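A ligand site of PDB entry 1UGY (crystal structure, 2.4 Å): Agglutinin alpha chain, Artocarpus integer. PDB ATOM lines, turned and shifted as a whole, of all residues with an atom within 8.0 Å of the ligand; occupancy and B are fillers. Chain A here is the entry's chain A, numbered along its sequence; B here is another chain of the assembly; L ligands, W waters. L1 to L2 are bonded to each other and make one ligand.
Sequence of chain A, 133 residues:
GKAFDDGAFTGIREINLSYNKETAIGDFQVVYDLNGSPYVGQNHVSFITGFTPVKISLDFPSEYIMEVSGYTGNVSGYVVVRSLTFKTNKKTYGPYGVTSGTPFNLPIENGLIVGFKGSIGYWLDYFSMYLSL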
ATOM      1  N   GLY A   1     -35.892 -23.054  21.843  1.00  0.00           N
ATOM      2  CA  GLY A   1     -35.569 -21.621  22.081  1.00  0.00           C
ATOM      3  C   GLY A   1     -36.780 -20.717  21.892  1.00  0.00           C
ATOM      4  O   GLY A   1     -37.911 -21.189  21.791  1.00  0.00           O
ATOM      5  N   LYS A   2     -36.534 -19.410  21.843  1.00  0.00           N
ATOM      6  CA  LYS A   2     -37.608 -18.446  21.655  1.00  0.00           C
ATOM      7  C   LYS A   2     -37.772 -18.147  20.170  1.00  0.00           C
ATOM      8  O   LYS A   2     -36.835 -17.723  19.496  1.00  0.00           O
ATOM      9  CB  LYS A   2     -37.295 -17.151  22.417  1.00  0.00           C
ATOM     10  CG  LYS A   2     -38.418 -16.136  22.369  1.00  0.00           C
ATOM     11  CD  LYS A   2     -38.073 -14.894  23.175  1.00  0.00           C
ATOM     12  CE  LYS A   2     -39.241 -13.909  23.187  1.00  0.00           C
ATOM     13  NZ  LYS A   2     -38.984 -12.707  24.043  1.00  0.00           N
ATOM     14  N   ALA A  24     -21.773 -22.406  17.594  1.00  0.00           N
ATOM     15  CA  ALA A  24     -22.723 -22.087  16.532  1.00  0.00           C
ATOM     16  C   ALA A  24     -23.066 -20.613  16.498  1.00  0.00           C
ATOM     17  O   ALA A  24     -22.415 -19.793  17.131  1.00  0.00           O
ATOM     18  CB  ALA A  24     -23.995 -22.905  16.730  1.00  0.00           C
ATOM     19  N   ILE A  25     -24.102 -20.274  15.726  1.00  0.00           N
ATOM     20  CA  ILE A  25     -24.540 -18.902  15.608  1.00  0.00           C
ATOM     21  C   ILE A  25     -25.353 -18.500  16.826  1.00  0.00           C
ATOM     22  O   ILE A  25     -26.177 -19.266  17.324  1.00  0.00           O
ATOM     23  CB  ILE A  25     -25.368 -18.737  14.333  1.00  0.00           C
ATOM     24  CG1 ILE A  25     -24.470 -18.987  13.127  1.00  0.00           C
ATOM     25  CG2 ILE A  25     -25.961 -17.333  14.250  1.00  0.00           C
ATOM     26  CD1 ILE A  25     -25.233 -19.383  11.915  1.00  0.00           C
ATOM     27  N   SER A  46     -29.216 -14.380  22.013  1.00  0.00           N
ATOM     28  CA  SER A  46     -28.992 -15.717  22.550  1.00  0.00           C
ATOM     29  C   SER A  46     -29.203 -15.694  24.058  1.00  0.00           C
ATOM     30  O   SER A  46     -29.003 -14.655  24.703  1.00  0.00           O
ATOM     31  CB  SER A  46     -27.557 -16.131  22.245  1.00  0.00           C
ATOM     32  OG  SER A  46     -27.179 -17.259  22.995  1.00  0.00           O
ATOM     33  N   PHE A  47     -29.602 -16.829  24.635  1.00  0.00           N
ATOM     34  CA  PHE A  47     -29.824 -16.887  26.081  1.00  0.00           C
ATOM     35  C   PHE A  47     -28.527 -16.649  26.844  1.00  0.00           C
ATOM     36  O   PHE A  47     -28.537 -16.210  27.989  1.00  0.00           O
ATOM     37  CB  PHE A  47     -30.396 -18.253  26.485  1.00  0.00           C
ATOM     38  CG  PHE A  47     -31.803 -18.512  26.010  1.00  0.00           C
ATOM     39  CD1 PHE A  47     -32.550 -17.506  25.398  1.00  0.00           C
ATOM     40  CD2 PHE A  47     -32.389 -19.765  26.182  1.00  0.00           C
ATOM     41  CE1 PHE A  47     -33.870 -17.743  24.974  1.00  0.00           C
ATOM     42  CE2 PHE A  47     -33.698 -20.011  25.761  1.00  0.00           C
ATOM     43  CZ  PHE A  47     -34.437 -19.004  25.155  1.00  0.00           C
ATOM     44  N   ILE A  48     -27.399 -16.941  26.193  1.00  0.00           N
ATOM     45  CA  ILE A  48     -26.088 -16.764  26.811  1.00  0.00           C
ATOM     46  C   ILE A  48     -25.280 -15.688  26.072  1.00  0.00           C
ATOM     47  O   ILE A  48     -25.785 -15.066  25.137  1.00  0.00           O
ATOM     48  CB  ILE A  48     -25.291 -18.081  26.807  1.00  0.00           C
ATOM     49  CG1 ILE A  48     -25.221 -18.644  25.380  1.00  0.00           C
ATOM     50  CG2 ILE A  48     -25.950 -19.093  27.744  1.00  0.00           C
ATOM     51  CD1 ILE A  48     -24.243 -19.772  25.214  1.00  0.00           C
ATOM     52  N   VAL A  75     -24.871 -29.571  18.998  1.00  0.00           N
ATOM     53  CA  VAL A  75     -24.086 -28.841  19.969  1.00  0.00           C
ATOM     54  C   VAL A  75     -24.811 -29.450  21.146  1.00  0.00           C
ATOM     55  O   VAL A  75     -25.984 -29.152  21.382  1.00  0.00           O
ATOM     56  CB  VAL A  75     -24.295 -27.310  19.889  1.00  0.00           C
ATOM     57  CG1 VAL A  75     -23.662 -26.638  21.091  1.00  0.00           C
ATOM     58  CG2 VAL A  75     -23.653 -26.780  18.611  1.00  0.00           C
ATOM     59  N   SER A  76     -24.139 -30.344  21.864  1.00  0.00           N
ATOM     60  CA  SER A  76     -24.771 -31.087  22.947  1.00  0.00           C
ATOM     61  C   SER A  76     -25.891 -31.868  22.246  1.00  0.00           C
ATOM     62  O   SER A  76     -25.696 -32.364  21.128  1.00  0.00           O
ATOM     63  CB  SER A  76     -25.350 -30.162  24.014  1.00  0.00           C
ATOM     64  OG  SER A  76     -24.330 -29.737  24.910  1.00  0.00           O
ATOM     65  N   GLY A  77     -27.059 -31.984  22.858  1.00  0.00           N
ATOM     66  CA  GLY A  77     -28.119 -32.731  22.210  1.00  0.00           C
ATOM     67  C   GLY A  77     -28.946 -32.030  21.130  1.00  0.00           C
ATOM     68  O   GLY A  77     -29.593 -32.692  20.337  1.00  0.00           O
ATOM     69  N   TYR A  78     -28.904 -30.706  21.083  1.00  0.00           N
ATOM     70  CA  TYR A  78     -29.685 -29.945  20.121  1.00  0.00           C
ATOM     71  C   TYR A  78     -29.105 -29.784  18.715  1.00  0.00           C
ATOM     72  O   TYR A  78     -27.894 -29.682  18.538  1.00  0.00           O
ATOM     73  CB  TYR A  78     -29.969 -28.553  20.702  1.00  0.00           C
ATOM     74  CG  TYR A  78     -30.565 -28.603  22.072  1.00  0.00           C
ATOM     75  CD1 TYR A  78     -31.916 -28.909  22.262  1.00  0.00           C
ATOM     76  CD2 TYR A  78     -29.779 -28.393  23.202  1.00  0.00           C
ATOM     77  CE1 TYR A  78     -32.455 -29.022  23.531  1.00  0.00           C
ATOM     78  CE2 TYR A  78     -30.306 -28.496  24.487  1.00  0.00           C
ATOM     79  CZ  TYR A  78     -31.645 -28.820  24.646  1.00  0.00           C
ATOM     80  OH  TYR A  78     -32.172 -28.963  25.918  1.00  0.00           O
ATOM     81  N   VAL A  79     -29.983 -29.753  17.724  1.00  0.00           N
ATOM     82  CA  VAL A  79     -29.574 -29.539  16.340  1.00  0.00           C
ATOM     83  C   VAL A  79     -29.690 -28.034  16.127  1.00  0.00           C
ATOM     84  O   VAL A  79     -30.722 -27.439  16.458  1.00  0.00           O
ATOM     85  CB  VAL A  79     -30.489 -30.271  15.341  1.00  0.00           C
ATOM     86  CG1 VAL A  79     -30.096 -29.887  13.918  1.00  0.00           C
ATOM     87  CG2 VAL A  79     -30.369 -31.775  15.500  1.00  0.00           C
ATOM     88  N   VAL A  80     -28.645 -27.413  15.596  1.00  0.00           N
ATOM     89  CA  VAL A  80     -28.659 -25.975  15.386  1.00  0.00           C
ATOM     90  C   VAL A  80     -27.920 -25.575  14.120  1.00  0.00           C
ATOM     91  O   VAL A  80     -27.354 -26.423  13.409  1.00  0.00           O
ATOM     92  CB  VAL A  80     -27.997 -25.244  16.579  1.00  0.00           C
ATOM     93  CG1 VAL A  80     -28.737 -25.577  17.876  1.00  0.00           C
ATOM     94  CG2 VAL A  80     -26.537 -25.651  16.697  1.00  0.00           C
ATOM     95  N   VAL A  81     -27.930 -24.274  13.832  1.00  0.00           N
ATOM     96  CA  VAL A  81     -27.245 -23.739  12.661  1.00  0.00           C
ATOM     97  C   VAL A  81     -25.851 -23.391  13.131  1.00  0.00           C
ATOM     98  O   VAL A  81     -25.652 -22.414  13.846  1.00  0.00           O
ATOM     99  CB  VAL A  81     -27.942 -22.475  12.133  1.00  0.00           C
ATOM    100  CG1 VAL A  81     -27.148 -21.885  10.982  1.00  0.00           C
ATOM    101  CG2 VAL A  81     -29.352 -22.842  11.668  1.00  0.00           C
ATOM    102  N   SER A 119     -35.778 -19.322  15.296  1.00  0.00           N
ATOM    103  CA  SER A 119     -35.765 -19.534  16.741  1.00  0.00           C
ATOM    104  C   SER A 119     -34.347 -19.526  17.281  1.00  0.00           C
ATOM    105  O   SER A 119     -33.419 -20.007  16.636  1.00  0.00           O
ATOM    106  CB  SER A 119     -36.431 -20.864  17.085  1.00  0.00           C
ATOM    107  OG  SER A 119     -36.260 -21.162  18.462  1.00  0.00           O
ATOM    108  N   ILE A 120     -34.188 -18.967  18.478  1.00  0.00           N
ATOM    109  CA  ILE A 120     -32.883 -18.889  19.110  1.00  0.00           C
ATOM    110  C   ILE A 120     -32.993 -19.166  20.603  1.00  0.00           C
ATOM    111  O   ILE A 120     -33.803 -18.549  21.300  1.00  0.00           O
ATOM    112  CB  ILE A 120     -32.256 -17.486  18.942  1.00  0.00           C
ATOM    113  CG1 ILE A 120     -32.114 -17.154  17.454  1.00  0.00           C
ATOM    114  CG2 ILE A 120     -30.913 -17.438  19.625  1.00  0.00           C
ATOM    115  CD1 ILE A 120     -31.703 -15.721  17.187  1.00  0.00           C
ATOM    116  N   GLY A 121     -32.187 -20.114  21.071  1.00  0.00           N
ATOM    117  CA  GLY A 121     -32.143 -20.450  22.484  1.00  0.00           C
ATOM    118  C   GLY A 121     -30.734 -20.051  22.899  1.00  0.00           C
ATOM    119  O   GLY A 121     -30.443 -18.860  23.061  1.00  0.00           O
ATOM    120  N   TYR A 122     -29.858 -21.039  23.051  1.00  0.00           N
ATOM    121  CA  TYR A 122     -28.470 -20.739  23.384  1.00  0.00           C
ATOM    122  C   TYR A 122     -27.839 -20.388  22.032  1.00  0.00           C
ATOM    123  O   TYR A 122     -26.925 -19.567  21.952  1.00  0.00           O
ATOM    124  CB  TYR A 122     -27.779 -21.954  23.983  1.00  0.00           C
ATOM    125  CG  TYR A 122     -27.813 -21.994  25.495  1.00  0.00           C
ATOM    126  CD1 TYR A 122     -28.906 -21.508  26.204  1.00  0.00           C
ATOM    127  CD2 TYR A 122     -26.751 -22.542  26.215  1.00  0.00           C
ATOM    128  CE1 TYR A 122     -28.950 -21.566  27.584  1.00  0.00           C
ATOM    129  CE2 TYR A 122     -26.793 -22.604  27.607  1.00  0.00           C
ATOM    130  CZ  TYR A 122     -27.896 -22.118  28.280  1.00  0.00           C
ATOM    131  OH  TYR A 122     -27.945 -22.181  29.667  1.00  0.00           O
ATOM    132  N   TRP A 123     -28.350 -21.032  20.982  1.00  0.00           N
ATOM    133  CA  TRP A 123     -27.866 -20.832  19.616  1.00  0.00           C
ATOM    134  C   TRP A 123     -29.058 -20.750  18.667  1.00  0.00           C
ATOM    135  O   TRP A 123     -30.198 -20.976  19.069  1.00  0.00           O
ATOM    136  CB  TRP A 123     -26.963 -21.988  19.205  1.00  0.00           C
ATOM    137  CG  TRP A 123     -25.834 -22.199  20.161  1.00  0.00           C
ATOM    138  CD1 TRP A 123     -24.719 -21.428  20.298  1.00  0.00           C
ATOM    139  CD2 TRP A 123     -25.774 -23.185  21.199  1.00  0.00           C
ATOM    140  NE1 TRP A 123     -23.972 -21.869  21.367  1.00  0.00           N
ATOM    141  CE2 TRP A 123     -24.594 -22.943  21.934  1.00  0.00           C
ATOM    142  CE3 TRP A 123     -26.602 -24.250  21.589  1.00  0.00           C
ATOM    143  CZ2 TRP A 123     -24.219 -23.730  23.044  1.00  0.00           C
ATOM    144  CZ3 TRP A 123     -26.240 -25.024  22.684  1.00  0.00           C
ATOM    145  CH2 TRP A 123     -25.058 -24.751  23.398  1.00  0.00           C
ATOM    146  N   LEU A 124     -28.789 -20.431  17.406  1.00  0.00           N
ATOM    147  CA  LEU A 124     -29.838 -20.333  16.404  1.00  0.00           C
ATOM    148  C   LEU A 124     -30.343 -21.743  16.088  1.00  0.00           C
ATOM    149  O   LEU A 124     -29.672 -22.506  15.401  1.00  0.00           O
ATOM    150  CB  LEU A 124     -29.275 -19.677  15.138  1.00  0.00           C
ATOM    151  CG  LEU A 124     -30.196 -19.557  13.919  1.00  0.00           C
ATOM    152  CD1 LEU A 124     -31.425 -18.711  14.245  1.00  0.00           C
ATOM    153  CD2 LEU A 124     -29.398 -18.935  12.777  1.00  0.00           C
ATOM    154  N   ASP A 125     -31.533 -22.075  16.594  1.00  0.00           N
ATOM    155  CA  ASP A 125     -32.116 -23.402  16.391  1.00  0.00           C
ATOM    156  C   ASP A 125     -32.439 -23.720  14.936  1.00  0.00           C
ATOM    157  O   ASP A 125     -32.185 -24.823  14.459  1.00  0.00           O
ATOM    158  CB  ASP A 125     -33.388 -23.565  17.221  1.00  0.00           C
ATOM    159  CG  ASP A 125     -33.172 -23.297  18.704  1.00  0.00           C
ATOM    160  OD1 ASP A 125     -32.262 -23.906  19.296  1.00  0.00           O
ATOM    161  OD2 ASP A 125     -33.938 -22.485  19.268  1.00  0.00           O
ATOM    162  N   TYR A 126     -33.025 -22.754  14.232  1.00  0.00           N
ATOM    163  CA  TYR A 126     -33.405 -22.937  12.841  1.00  0.00           C
ATOM    164  C   TYR A 126     -33.909 -21.610  12.273  1.00  0.00           C
ATOM    165  O   TYR A 126     -34.182 -20.685  13.028  1.00  0.00           O
ATOM    166  CB  TYR A 126     -34.517 -23.981  12.733  1.00  0.00           C
ATOM    167  CG  TYR A 126     -35.809 -23.590  13.442  1.00  0.00           C
ATOM    168  CD1 TYR A 126     -36.692 -22.676  12.879  1.00  0.00           C
ATOM    169  CD2 TYR A 126     -36.142 -24.140  14.682  1.00  0.00           C
ATOM    170  CE1 TYR A 126     -37.871 -22.310  13.527  1.00  0.00           C
ATOM    171  CE2 TYR A 126     -37.316 -23.787  15.340  1.00  0.00           C
ATOM    172  CZ  TYR A 126     -38.168 -22.876  14.755  1.00  0.00           C
ATOM    173  OH  TYR A 126     -39.331 -22.532  15.415  1.00  0.00           O
ATOM    174  N   ALA B  17     -33.082 -27.381  13.394  1.00  0.00           N
ATOM    175  CA  ALA B  17     -33.920 -28.324  14.116  1.00  0.00           C
ATOM    176  C   ALA B  17     -35.329 -28.399  13.552  1.00  0.00           C
ATOM    177  O   ALA B  17     -35.819 -27.442  12.955  1.00  0.00           O
ATOM    178  CB  ALA B  17     -33.979 -27.957  15.589  1.00  0.00           C
HETATM  179  C1  LIG L   1     -27.690 -27.381  28.003  1.00  0.00           C
HETATM  180  C2  LIG L   1     -27.640 -26.600  29.313  1.00  0.00           C
HETATM  181  C3  LIG L   1     -29.035 -26.018  29.606  1.00  0.00           C
HETATM  182  C4  LIG L   1     -29.566 -25.234  28.420  1.00  0.00           C
HETATM  183  C5  LIG L   1     -29.361 -25.970  27.089  1.00  0.00           C
HETATM  184  C6  LIG L   1     -29.620 -25.034  25.968  1.00  0.00           C
HETATM  185  O1  LIG L   1     -26.462 -27.962  27.729  1.00  0.00           O
HETATM  186  O2  LIG L   1     -27.224 -27.443  30.373  1.00  0.00           O
HETATM  187  O3  LIG L   1     -28.975 -25.160  30.735  1.00  0.00           O
HETATM  188  O4  LIG L   1     -30.962 -25.019  28.604  1.00  0.00           O
HETATM  189  O5  LIG L   1     -28.022 -26.462  26.944  1.00  0.00           O
HETATM  190  O6  LIG L   1     -31.003 -25.177  25.619  1.00  0.00           O
HETATM  191  C1  LG2 L   2     -31.514 -24.056  24.991  1.00  0.00           C
HETATM  192  C2  LG2 L   2     -33.026 -24.220  24.858  1.00  0.00           C
HETATM  193  C3  LG2 L   2     -33.359 -25.294  23.847  1.00  0.00           C
HETATM  194  C4  LG2 L   2     -32.627 -25.042  22.518  1.00  0.00           C
HETATM  195  C5  LG2 L   2     -31.122 -24.897  22.775  1.00  0.00           C
HETATM  196  C6  LG2 L   2     -30.261 -24.647  21.540  1.00  0.00           C
HETATM  197  O1  LG2 L   2     -33.561 -24.579  26.120  1.00  0.00           O
HETATM  198  O2  LG2 L   2     -34.776 -25.345  23.634  1.00  0.00           O
HETATM  199  O3  LG2 L   2     -33.150 -23.867  21.917  1.00  0.00           O
HETATM  200  O4  LG2 L   2     -30.895 -23.836  23.726  1.00  0.00           O
HETATM  201  O5  LG2 L   2     -30.278 -23.288  21.160  1.00  0.00           O
HETATM  202  O   HOH W   1     -35.997 -27.027  21.844  1.00  0.00           O
HETATM  203  O   HOH W   2     -25.075 -30.634  27.825  1.00  0.00           O
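The backbone NH (N) of Tyr 122 is in hydrogen-bond range of an oxygen (O5) of LG2 L2.
OH of Tyr 122 sits at hydrogen-bond distance from O3 of LIG L1 (3.3 Å).
OD1 of Asp 125 is in hydrogen-bond range of O3 of LG2 L2, 2.8 Å away.
O5 of LG2 L2 sits at hydrogen-bond distance from O of Trp 123 (3.1 Å).
The backbone NH of Trp 123 is in hydrogen-bond range of an oxygen (O5) of LG2 L2.
O3 of LG2 L2 is in hydrogen-bond range of N of Gly 1, at 2.9 Å.
The side-chain carboxylate (OD2) of Asp 125 sits at hydrogen-bond distance from the backbone NH (N) of Gly 1 (3.3 Å).
The side-chain hydroxyl of Ser 119 is in hydrogen-bond range of the side-chain carboxylate of Asp 125 (2.8 Å).
OD2 of Asp 125 sits at hydrogen-bond distance from N of Gly 121, at 3.5 Å.
The backbone carbonyl oxygen of Gly 121 lies within hydrogen-bond range of the backbone NH of Phe 47 (2.7 Å).
The backbone carbonyl oxygen of Tyr 122 lies within hydrogen-bond range of the side-chain hydroxyl of Ser 46 (2.5 Å).
The backbone carbonyl oxygen of Asp 125 lies within hydrogen-bond range of the backbone NH of Ala 17 of chain B, at 2.9 Å.
Residues that only touch the ligand: Ser 76 (3.96 Å), Tyr 78 (3.6 Å) and Gly 121 (3.6 Å).
Seven residues have an atom within 4 Å of the ligand: Gly 1, Ser 76, Tyr 78, Gly 121, Tyr 122, Trp 123 and Asp 125.
Along chain A the residues within 4 Å of the ligand span positions 1 to 125.
Water W2 lies within hydrogen-bond range of an oxygen (O1) of LIG L1 (3.0 Å) and the side-chain hydroxyl (OG) of Ser 76 (3.1 Å).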
